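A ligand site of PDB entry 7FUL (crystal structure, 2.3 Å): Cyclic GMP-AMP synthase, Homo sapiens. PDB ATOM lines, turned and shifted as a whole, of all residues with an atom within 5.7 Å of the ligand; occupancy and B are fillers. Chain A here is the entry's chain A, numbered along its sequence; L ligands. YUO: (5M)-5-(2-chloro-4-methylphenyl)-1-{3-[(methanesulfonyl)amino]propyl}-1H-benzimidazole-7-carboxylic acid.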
ATOM      1  N   LYS A  59      17.484   4.766   2.358  1.00  0.00           N
ATOM      2  CA  LYS A  59      17.393   6.077   3.006  1.00  0.00           C
ATOM      3  C   LYS A  59      16.039   6.223   3.697  1.00  0.00           C
ATOM      4  O   LYS A  59      15.015   5.751   3.185  1.00  0.00           O
ATOM      5  CB  LYS A  59      17.607   7.185   1.960  1.00  0.00           C
ATOM      6  CG  LYS A  59      17.399   8.617   2.438  1.00  0.00           C
ATOM      7  CD  LYS A  59      17.313   9.607   1.264  1.00  0.00           C
ATOM      8  CE  LYS A  59      18.652   9.754   0.544  1.00  0.00           C
ATOM      9  NZ  LYS A  59      19.017  11.178   0.178  1.00  0.00           N
ATOM     10  N   ASP A  67      13.287   5.384   1.204  1.00  0.00           N
ATOM     11  CA  ASP A  67      13.577   5.761  -0.181  1.00  0.00           C
ATOM     12  C   ASP A  67      14.767   4.958  -0.685  1.00  0.00           C
ATOM     13  O   ASP A  67      15.817   4.918  -0.044  1.00  0.00           O
ATOM     14  CB  ASP A  67      13.834   7.268  -0.298  1.00  0.00           C
ATOM     15  CG  ASP A  67      12.531   8.076  -0.418  1.00  0.00           C
ATOM     16  OD1 ASP A  67      11.454   7.559  -0.064  1.00  0.00           O
ATOM     17  OD2 ASP A  67      12.572   9.240  -0.882  1.00  0.00           O
ATOM     18  N   PRO A 146       7.250  10.434  -9.538  1.00  0.00           N
ATOM     19  CA  PRO A 146       8.584  10.052 -10.019  1.00  0.00           C
ATOM     20  C   PRO A 146       8.977   8.668  -9.577  1.00  0.00           C
ATOM     21  O   PRO A 146       9.974   8.135 -10.061  1.00  0.00           O
ATOM     22  CB  PRO A 146       9.495  11.081  -9.345  1.00  0.00           C
ATOM     23  CG  PRO A 146       8.818  11.279  -8.013  1.00  0.00           C
ATOM     24  CD  PRO A 146       7.324  11.202  -8.276  1.00  0.00           C
ATOM     25  N   LEU A 178      25.836  23.876  -5.441  1.00  0.00           N
ATOM     26  CA  LEU A 178      26.834  23.229  -4.582  1.00  0.00           C
ATOM     27  C   LEU A 178      27.816  24.263  -4.041  1.00  0.00           C
ATOM     28  O   LEU A 178      29.033  24.148  -4.188  1.00  0.00           O
ATOM     29  CB  LEU A 178      27.582  22.114  -5.331  1.00  0.00           C
ATOM     30  CG  LEU A 178      28.384  21.098  -4.501  1.00  0.00           C
ATOM     31  CD1 LEU A 178      27.529  20.442  -3.446  1.00  0.00           C
ATOM     32  CD2 LEU A 178      28.962  20.023  -5.398  1.00  0.00           C
ATOM     33  N   VAL A 200      15.950  11.312 -13.156  1.00  0.00           N
ATOM     34  CA  VAL A 200      14.784  10.521 -12.797  1.00  0.00           C
ATOM     35  C   VAL A 200      13.616  10.986 -13.649  1.00  0.00           C
ATOM     36  O   VAL A 200      13.586  12.143 -14.109  1.00  0.00           O
ATOM     37  CB  VAL A 200      14.494  10.632 -11.302  1.00  0.00           C
ATOM     38  CG1 VAL A 200      15.744  10.301 -10.548  1.00  0.00           C
ATOM     39  CG2 VAL A 200      14.045  12.039 -10.973  1.00  0.00           C
ATOM     40  N   LYS A 202      10.720  12.291 -13.247  1.00  0.00           N
ATOM     41  CA  LYS A 202       9.728  13.194 -12.675  1.00  0.00           C
ATOM     42  C   LYS A 202       9.262  14.154 -13.762  1.00  0.00           C
ATOM     43  O   LYS A 202      10.069  14.847 -14.385  1.00  0.00           O
ATOM     44  CB  LYS A 202      10.291  13.988 -11.491  1.00  0.00           C
ATOM     45  CG  LYS A 202       9.472  15.239 -11.154  1.00  0.00           C
ATOM     46  CD  LYS A 202       9.586  15.604  -9.674  1.00  0.00           C
ATOM     47  CE  LYS A 202       8.496  16.588  -9.257  1.00  0.00           C
ATOM     48  NZ  LYS A 202       8.391  16.736  -7.771  1.00  0.00           N
ATOM     49  N   ARG A 216      14.050  14.697 -14.478  1.00  0.00           N
ATOM     50  CA  ARG A 216      14.587  15.619 -13.484  1.00  0.00           C
ATOM     51  C   ARG A 216      15.998  15.210 -13.097  1.00  0.00           C
ATOM     52  O   ARG A 216      16.273  14.017 -12.921  1.00  0.00           O
ATOM     53  CB  ARG A 216      13.703  15.640 -12.235  1.00  0.00           C
ATOM     54  CG  ARG A 216      14.178  16.616 -11.184  1.00  0.00           C
ATOM     55  CD  ARG A 216      13.071  17.105 -10.255  1.00  0.00           C
ATOM     56  NE  ARG A 216      13.665  17.727  -9.064  1.00  0.00           N
ATOM     57  CZ  ARG A 216      12.980  18.275  -8.057  1.00  0.00           C
ATOM     58  NH1 ARG A 216      11.650  18.303  -8.069  1.00  0.00           N
ATOM     59  NH2 ARG A 216      13.645  18.806  -7.039  1.00  0.00           N
ATOM     60  N   LEU A 217      16.885  16.187 -12.988  1.00  0.00           N
ATOM     61  CA  LEU A 217      18.227  15.955 -12.447  1.00  0.00           C
ATOM     62  C   LEU A 217      18.176  15.612 -10.960  1.00  0.00           C
ATOM     63  O   LEU A 217      17.389  16.194 -10.211  1.00  0.00           O
ATOM     64  CB  LEU A 217      19.114  17.186 -12.625  1.00  0.00           C
ATOM     65  CG  LEU A 217      19.529  17.659 -13.992  1.00  0.00           C
ATOM     66  CD1 LEU A 217      20.455  18.820 -13.819  1.00  0.00           C
ATOM     67  CD2 LEU A 217      20.237  16.541 -14.679  1.00  0.00           C
ATOM     68  N   SER A 218      19.052  14.705 -10.532  1.00  0.00           N
ATOM     69  CA  SER A 218      19.033  14.235  -9.153  1.00  0.00           C
ATOM     70  C   SER A 218      20.443  14.127  -8.594  1.00  0.00           C
ATOM     71  O   SER A 218      21.302  13.469  -9.176  1.00  0.00           O
ATOM     72  CB  SER A 218      18.351  12.870  -9.044  1.00  0.00           C
ATOM     73  OG  SER A 218      18.158  12.512  -7.676  1.00  0.00           O
ATOM     74  N   PHE A 219      20.645  14.729  -7.427  1.00  0.00           N
ATOM     75  CA  PHE A 219      21.926  14.661  -6.737  1.00  0.00           C
ATOM     76  C   PHE A 219      21.797  14.045  -5.339  1.00  0.00           C
ATOM     77  O   PHE A 219      22.686  14.223  -4.498  1.00  0.00           O
ATOM     78  CB  PHE A 219      22.545  16.059  -6.668  1.00  0.00           C
ATOM     79  CG  PHE A 219      22.816  16.656  -8.035  1.00  0.00           C
ATOM     80  CD1 PHE A 219      24.024  16.387  -8.705  1.00  0.00           C
ATOM     81  CD2 PHE A 219      21.866  17.475  -8.652  1.00  0.00           C
ATOM     82  CE1 PHE A 219      24.278  16.933  -9.963  1.00  0.00           C
ATOM     83  CE2 PHE A 219      22.121  18.027  -9.902  1.00  0.00           C
ATOM     84  CZ  PHE A 219      23.337  17.759 -10.561  1.00  0.00           C
ATOM     85  N   SER A 220      20.691  13.353  -5.084  1.00  0.00           N
ATOM     86  CA  SER A 220      20.402  12.685  -3.825  1.00  0.00           C
ATOM     87  C   SER A 220      21.611  11.929  -3.290  1.00  0.00           C
ATOM     88  O   SER A 220      21.875  11.928  -2.081  1.00  0.00           O
ATOM     89  CB  SER A 220      19.226  11.720  -4.027  1.00  0.00           C
ATOM     90  OG  SER A 220      19.211  10.723  -3.026  1.00  0.00           O
ATOM     91  N   HIS A 221      22.375  11.310  -4.173  1.00  0.00           N
ATOM     92  CA  HIS A 221      23.514  10.517  -3.752  1.00  0.00           C
ATOM     93  C   HIS A 221      24.636  11.360  -3.155  1.00  0.00           C
ATOM     94  O   HIS A 221      25.587  10.792  -2.613  1.00  0.00           O
ATOM     95  CB  HIS A 221      24.064   9.731  -4.932  1.00  0.00           C
ATOM     96  CG  HIS A 221      24.564  10.602  -6.040  1.00  0.00           C
ATOM     97  ND1 HIS A 221      23.792  11.595  -6.608  1.00  0.00           N
ATOM     98  CD2 HIS A 221      25.752  10.636  -6.681  1.00  0.00           C
ATOM     99  CE1 HIS A 221      24.479  12.202  -7.557  1.00  0.00           C
ATOM    100  NE2 HIS A 221      25.670  11.641  -7.621  1.00  0.00           N
ATOM    101  N   ILE A 222      24.574  12.693  -3.298  1.00  0.00           N
ATOM    102  CA  ILE A 222      25.641  13.534  -2.729  1.00  0.00           C
ATOM    103  C   ILE A 222      25.437  13.733  -1.230  1.00  0.00           C
ATOM    104  O   ILE A 222      26.406  14.008  -0.508  1.00  0.00           O
ATOM    105  CB  ILE A 222      25.719  14.877  -3.477  1.00  0.00           C
ATOM    106  CG1 ILE A 222      25.855  14.682  -4.994  1.00  0.00           C
ATOM    107  CG2 ILE A 222      26.898  15.708  -3.010  1.00  0.00           C
ATOM    108  CD1 ILE A 222      27.146  14.058  -5.440  1.00  0.00           C
ATOM    109  N   GLU A 223      24.219  13.540  -0.727  1.00  0.00           N
ATOM    110  CA  GLU A 223      23.926  13.864   0.672  1.00  0.00           C
ATOM    111  C   GLU A 223      24.848  13.112   1.629  1.00  0.00           C
ATOM    112  O   GLU A 223      25.449  13.716   2.521  1.00  0.00           O
ATOM    113  CB  GLU A 223      22.474  13.574   0.980  1.00  0.00           C
ATOM    114  CG  GLU A 223      22.052  14.085   2.351  1.00  0.00           C
ATOM    115  CD  GLU A 223      20.662  13.629   2.759  1.00  0.00           C
ATOM    116  OE1 GLU A 223      20.009  12.904   1.976  1.00  0.00           O
ATOM    117  OE2 GLU A 223      20.231  14.025   3.861  1.00  0.00           O
ATOM    118  N   ILE A 226      28.366  14.393   2.070  1.00  0.00           N
ATOM    119  CA  ILE A 226      28.556  15.628   2.812  1.00  0.00           C
ATOM    120  C   ILE A 226      28.064  15.512   4.253  1.00  0.00           C
ATOM    121  O   ILE A 226      28.668  16.077   5.163  1.00  0.00           O
ATOM    122  CB  ILE A 226      27.862  16.780   2.076  1.00  0.00           C
ATOM    123  CG1 ILE A 226      28.564  17.016   0.737  1.00  0.00           C
ATOM    124  CG2 ILE A 226      27.746  18.015   2.999  1.00  0.00           C
ATOM    125  CD1 ILE A 226      28.039  18.199  -0.013  1.00  0.00           C
ATOM    126  N   TYR A 276      12.887  16.685   2.184  1.00  0.00           N
ATOM    127  CA  TYR A 276      13.762  17.221   1.157  1.00  0.00           C
ATOM    128  C   TYR A 276      13.922  18.732   1.314  1.00  0.00           C
ATOM    129  O   TYR A 276      15.036  19.255   1.222  1.00  0.00           O
ATOM    130  CB  TYR A 276      13.219  16.871  -0.226  1.00  0.00           C
ATOM    131  CG  TYR A 276      13.953  17.488  -1.400  1.00  0.00           C
ATOM    132  CD1 TYR A 276      15.346  17.479  -1.479  1.00  0.00           C
ATOM    133  CD2 TYR A 276      13.251  18.053  -2.462  1.00  0.00           C
ATOM    134  CE1 TYR A 276      16.006  18.030  -2.587  1.00  0.00           C
ATOM    135  CE2 TYR A 276      13.897  18.603  -3.567  1.00  0.00           C
ATOM    136  CZ  TYR A 276      15.265  18.589  -3.625  1.00  0.00           C
ATOM    137  OH  TYR A 276      15.905  19.134  -4.724  1.00  0.00           O
ATOM    138  N   LYS A 279      16.139  19.249   4.562  1.00  0.00           N
ATOM    139  CA  LYS A 279      17.550  19.032   4.206  1.00  0.00           C
ATOM    140  C   LYS A 279      18.126  20.229   3.470  1.00  0.00           C
ATOM    141  O   LYS A 279      19.197  20.740   3.839  1.00  0.00           O
ATOM    142  CB  LYS A 279      17.687  17.794   3.321  1.00  0.00           C
ATOM    143  CG  LYS A 279      17.430  16.459   3.987  1.00  0.00           C
ATOM    144  CD  LYS A 279      17.477  15.370   2.916  1.00  0.00           C
ATOM    145  CE  LYS A 279      17.087  14.018   3.436  1.00  0.00           C
ATOM    146  NZ  LYS A 279      16.670  13.198   2.261  1.00  0.00           N
ATOM    147  N   THR A 280      17.420  20.690   2.428  1.00  0.00           N
ATOM    148  CA  THR A 280      17.902  21.768   1.558  1.00  0.00           C
ATOM    149  C   THR A 280      18.120  23.063   2.337  1.00  0.00           C
ATOM    150  O   THR A 280      19.156  23.725   2.171  1.00  0.00           O
ATOM    151  CB  THR A 280      16.889  21.998   0.429  1.00  0.00           C
ATOM    152  OG1 THR A 280      16.756  20.802  -0.355  1.00  0.00           O
ATOM    153  CG2 THR A 280      17.334  23.124  -0.488  1.00  0.00           C
ATOM    154  N   PHE A 283      21.295  22.594   4.605  1.00  0.00           N
ATOM    155  CA  PHE A 283      22.586  22.778   3.941  1.00  0.00           C
ATOM    156  C   PHE A 283      22.824  24.211   3.459  1.00  0.00           C
ATOM    157  O   PHE A 283      23.974  24.636   3.364  1.00  0.00           O
ATOM    158  CB  PHE A 283      22.717  21.812   2.782  1.00  0.00           C
ATOM    159  CG  PHE A 283      22.910  20.396   3.219  1.00  0.00           C
ATOM    160  CD1 PHE A 283      24.103  20.014   3.803  1.00  0.00           C
ATOM    161  CD2 PHE A 283      21.883  19.468   3.093  1.00  0.00           C
ATOM    162  CE1 PHE A 283      24.292  18.695   4.226  1.00  0.00           C
ATOM    163  CE2 PHE A 283      22.079  18.155   3.510  1.00  0.00           C
ATOM    164  CZ  PHE A 283      23.291  17.772   4.079  1.00  0.00           C
ATOM    165  N   ASN A 322      16.775  24.962  -4.935  1.00  0.00           N
ATOM    166  CA  ASN A 322      17.487  23.715  -5.100  1.00  0.00           C
ATOM    167  C   ASN A 322      18.983  23.915  -4.821  1.00  0.00           C
ATOM    168  O   ASN A 322      19.613  24.817  -5.377  1.00  0.00           O
ATOM    169  CB  ASN A 322      17.256  23.207  -6.510  1.00  0.00           C
ATOM    170  CG  ASN A 322      17.756  21.821  -6.709  1.00  0.00           C
ATOM    171  OD1 ASN A 322      18.956  21.573  -6.665  1.00  0.00           O
ATOM    172  ND2 ASN A 322      16.834  20.903  -6.977  1.00  0.00           N
ATOM    173  N   TYR A 323      19.525  23.087  -3.947  1.00  0.00           N
ATOM    174  CA  TYR A 323      20.901  23.238  -3.491  1.00  0.00           C
ATOM    175  C   TYR A 323      21.895  23.048  -4.607  1.00  0.00           C
ATOM    176  O   TYR A 323      23.025  23.547  -4.525  1.00  0.00           O
ATOM    177  CB  TYR A 323      21.200  22.225  -2.372  1.00  0.00           C
ATOM    178  CG  TYR A 323      22.390  22.591  -1.566  1.00  0.00           C
ATOM    179  CD1 TYR A 323      22.331  23.673  -0.696  1.00  0.00           C
ATOM    180  CD2 TYR A 323      23.582  21.893  -1.674  1.00  0.00           C
ATOM    181  CE1 TYR A 323      23.411  24.034   0.055  1.00  0.00           C
ATOM    182  CE2 TYR A 323      24.683  22.242  -0.930  1.00  0.00           C
ATOM    183  CZ  TYR A 323      24.586  23.324  -0.067  1.00  0.00           C
ATOM    184  OH  TYR A 323      25.658  23.709   0.717  1.00  0.00           O
ATOM    185  N   PHE A 324      21.507  22.329  -5.647  1.00  0.00           N
ATOM    186  CA  PHE A 324      22.358  22.134  -6.801  1.00  0.00           C
ATOM    187  C   PHE A 324      21.954  22.990  -7.995  1.00  0.00           C
ATOM    188  O   PHE A 324      22.765  23.156  -8.904  1.00  0.00           O
ATOM    189  CB  PHE A 324      22.364  20.663  -7.201  1.00  0.00           C
ATOM    190  CG  PHE A 324      22.927  19.779  -6.127  1.00  0.00           C
ATOM    191  CD1 PHE A 324      22.164  19.405  -5.031  1.00  0.00           C
ATOM    192  CD2 PHE A 324      24.251  19.340  -6.209  1.00  0.00           C
ATOM    193  CE1 PHE A 324      22.699  18.602  -4.033  1.00  0.00           C
ATOM    194  CE2 PHE A 324      24.794  18.549  -5.209  1.00  0.00           C
ATOM    195  CZ  PHE A 324      24.020  18.168  -4.130  1.00  0.00           C
HETATM  196  C10 YUO L   1      18.758  15.438  -1.038  1.00  0.00           C
HETATM  197  C11 YUO L   1      17.615  14.793  -1.494  1.00  0.00           C
HETATM  198  C13 YUO L   1      15.789  13.696  -1.687  1.00  0.00           C
HETATM  199  C15 YUO L   1      15.364  13.680  -4.170  1.00  0.00           C
HETATM  200  C16 YUO L   1      14.883  14.884  -4.959  1.00  0.00           C
HETATM  201  C17 YUO L   1      13.524  15.393  -4.577  1.00  0.00           C
HETATM  202  C20 YUO L   1      11.437  13.237  -4.786  1.00  0.00           C
HETATM  203  C23 YUO L   1      17.316  14.761  -2.864  1.00  0.00           C
HETATM  204  C24 YUO L   1      18.191  15.392  -3.760  1.00  0.00           C
HETATM  205  C25 YUO L   1      18.073  15.478  -5.243  1.00  0.00           C
HETATM  206  C28 YUO L   1      19.339  16.044  -3.272  1.00  0.00           C
HETATM  207  C1  YUO L   1      24.390  18.743   0.106  1.00  0.00           C
HETATM  208  C2  YUO L   1      23.157  18.058  -0.419  1.00  0.00           C
HETATM  209  C3  YUO L   1      21.908  18.609  -0.233  1.00  0.00           C
HETATM  210  C4  YUO L   1      20.775  17.981  -0.717  1.00  0.00           C
HETATM  211  C6  YUO L   1      20.852  16.771  -1.407  1.00  0.00           C
HETATM  212  C7  YUO L   1      22.116  16.209  -1.587  1.00  0.00           C
HETATM  213  C8  YUO L   1      23.249  16.855  -1.104  1.00  0.00           C
HETATM  214  C9  YUO L   1      19.636  16.064  -1.917  1.00  0.00           C
HETATM  215  N12 YUO L   1      16.630  14.103  -0.779  1.00  0.00           N
HETATM  216  N14 YUO L   1      16.126  14.051  -2.972  1.00  0.00           N
HETATM  217  N18 YUO L   1      12.661  15.455  -5.762  1.00  0.00           N
HETATM  218  O21 YUO L   1      10.670  14.564  -6.866  1.00  0.00           O
HETATM  219  O22 YUO L   1      12.804  13.351  -6.982  1.00  0.00           O
HETATM  220  O26 YUO L   1      18.393  16.499  -5.846  1.00  0.00           O
HETATM  221  O27 YUO L   1      17.665  14.393  -5.826  1.00  0.00           O
HETATM  222  S19 YUO L   1      11.871  14.127  -6.238  1.00  0.00           S
HETATM  223 CL5  YUO L   1      19.248  18.747  -0.427  1.00  0.00          CL
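Merely in contact with the ligand: Lys 59 (3.9 Å), Pro 146 (3.9 Å), Arg 216 (3.6 Å), Ile 222 (3.8 Å), Glu 223 (3.5 Å), Ile 226 (3.7 Å), Tyr 276 (3.4 Å), Thr 280 (3.2 Å), Phe 283 (3.4 Å), Tyr 323 (3.7 Å) and Phe 324 (3.4 Å).
16 residues have an atom within 4 Å of the ligand: Lys 59, Pro 146, Lys 202, Arg 216, Ser 218, Phe 219, Ser 220, Ile 222, Glu 223, Ile 226, Tyr 276, Lys 279, Thr 280, Phe 283, Tyr 323 and Phe 324.
OG of Ser 218 is in hydrogen-bond range of O27 of the ligand (2.7 Å).
The side-chain amino group of Lys 279 lies within hydrogen-bond range of a nitrogen (N12) of the ligand (3.2 Å).
The side-chain amino group of Lys 202 sits close to an oxygen (O21) of the ligand.
N of Phe 219 lies within hydrogen-bond range of O26 of the ligand (3.3 Å).
N of Ser 220 lies within hydrogen-bond range of O27 of the ligand (3.3 Å).
The side-chain amino group of Lys 279 is in salt-bridge range of the side-chain carboxylate of Glu 223 (3.4 Å).
The backbone carbonyl oxygen of Tyr 276 lies within hydrogen-bond range of the side-chain hydroxyl of Thr 280 (2.8 Å).
The side-chain hydroxyl of Ser 220 lies within hydrogen-bond range of the side-chain amino group of Lys 59, at 3.2 Å.
The backbone NH (N) of Phe 324 is in hydrogen-bond range of the side-chain amide oxygen (OD1) of Asn 322, at 2.8 Å.
The backbone carbonyl oxygen (O) of Phe 283 is in hydrogen-bond range of the side-chain hydroxyl (OH) of Tyr 323 (3.3 Å).
NZ of Lys 59 lies within salt-bridge range of OE1 of Glu 223 (2.7 Å).
N of Arg 216 sits at hydrogen-bond distance from O of Val 200 (2.6 Å).
The backbone NH (N) of Asp 67 lies within hydrogen-bond range of the backbone carbonyl oxygen (O) of Lys 59, 2.7 Å away.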
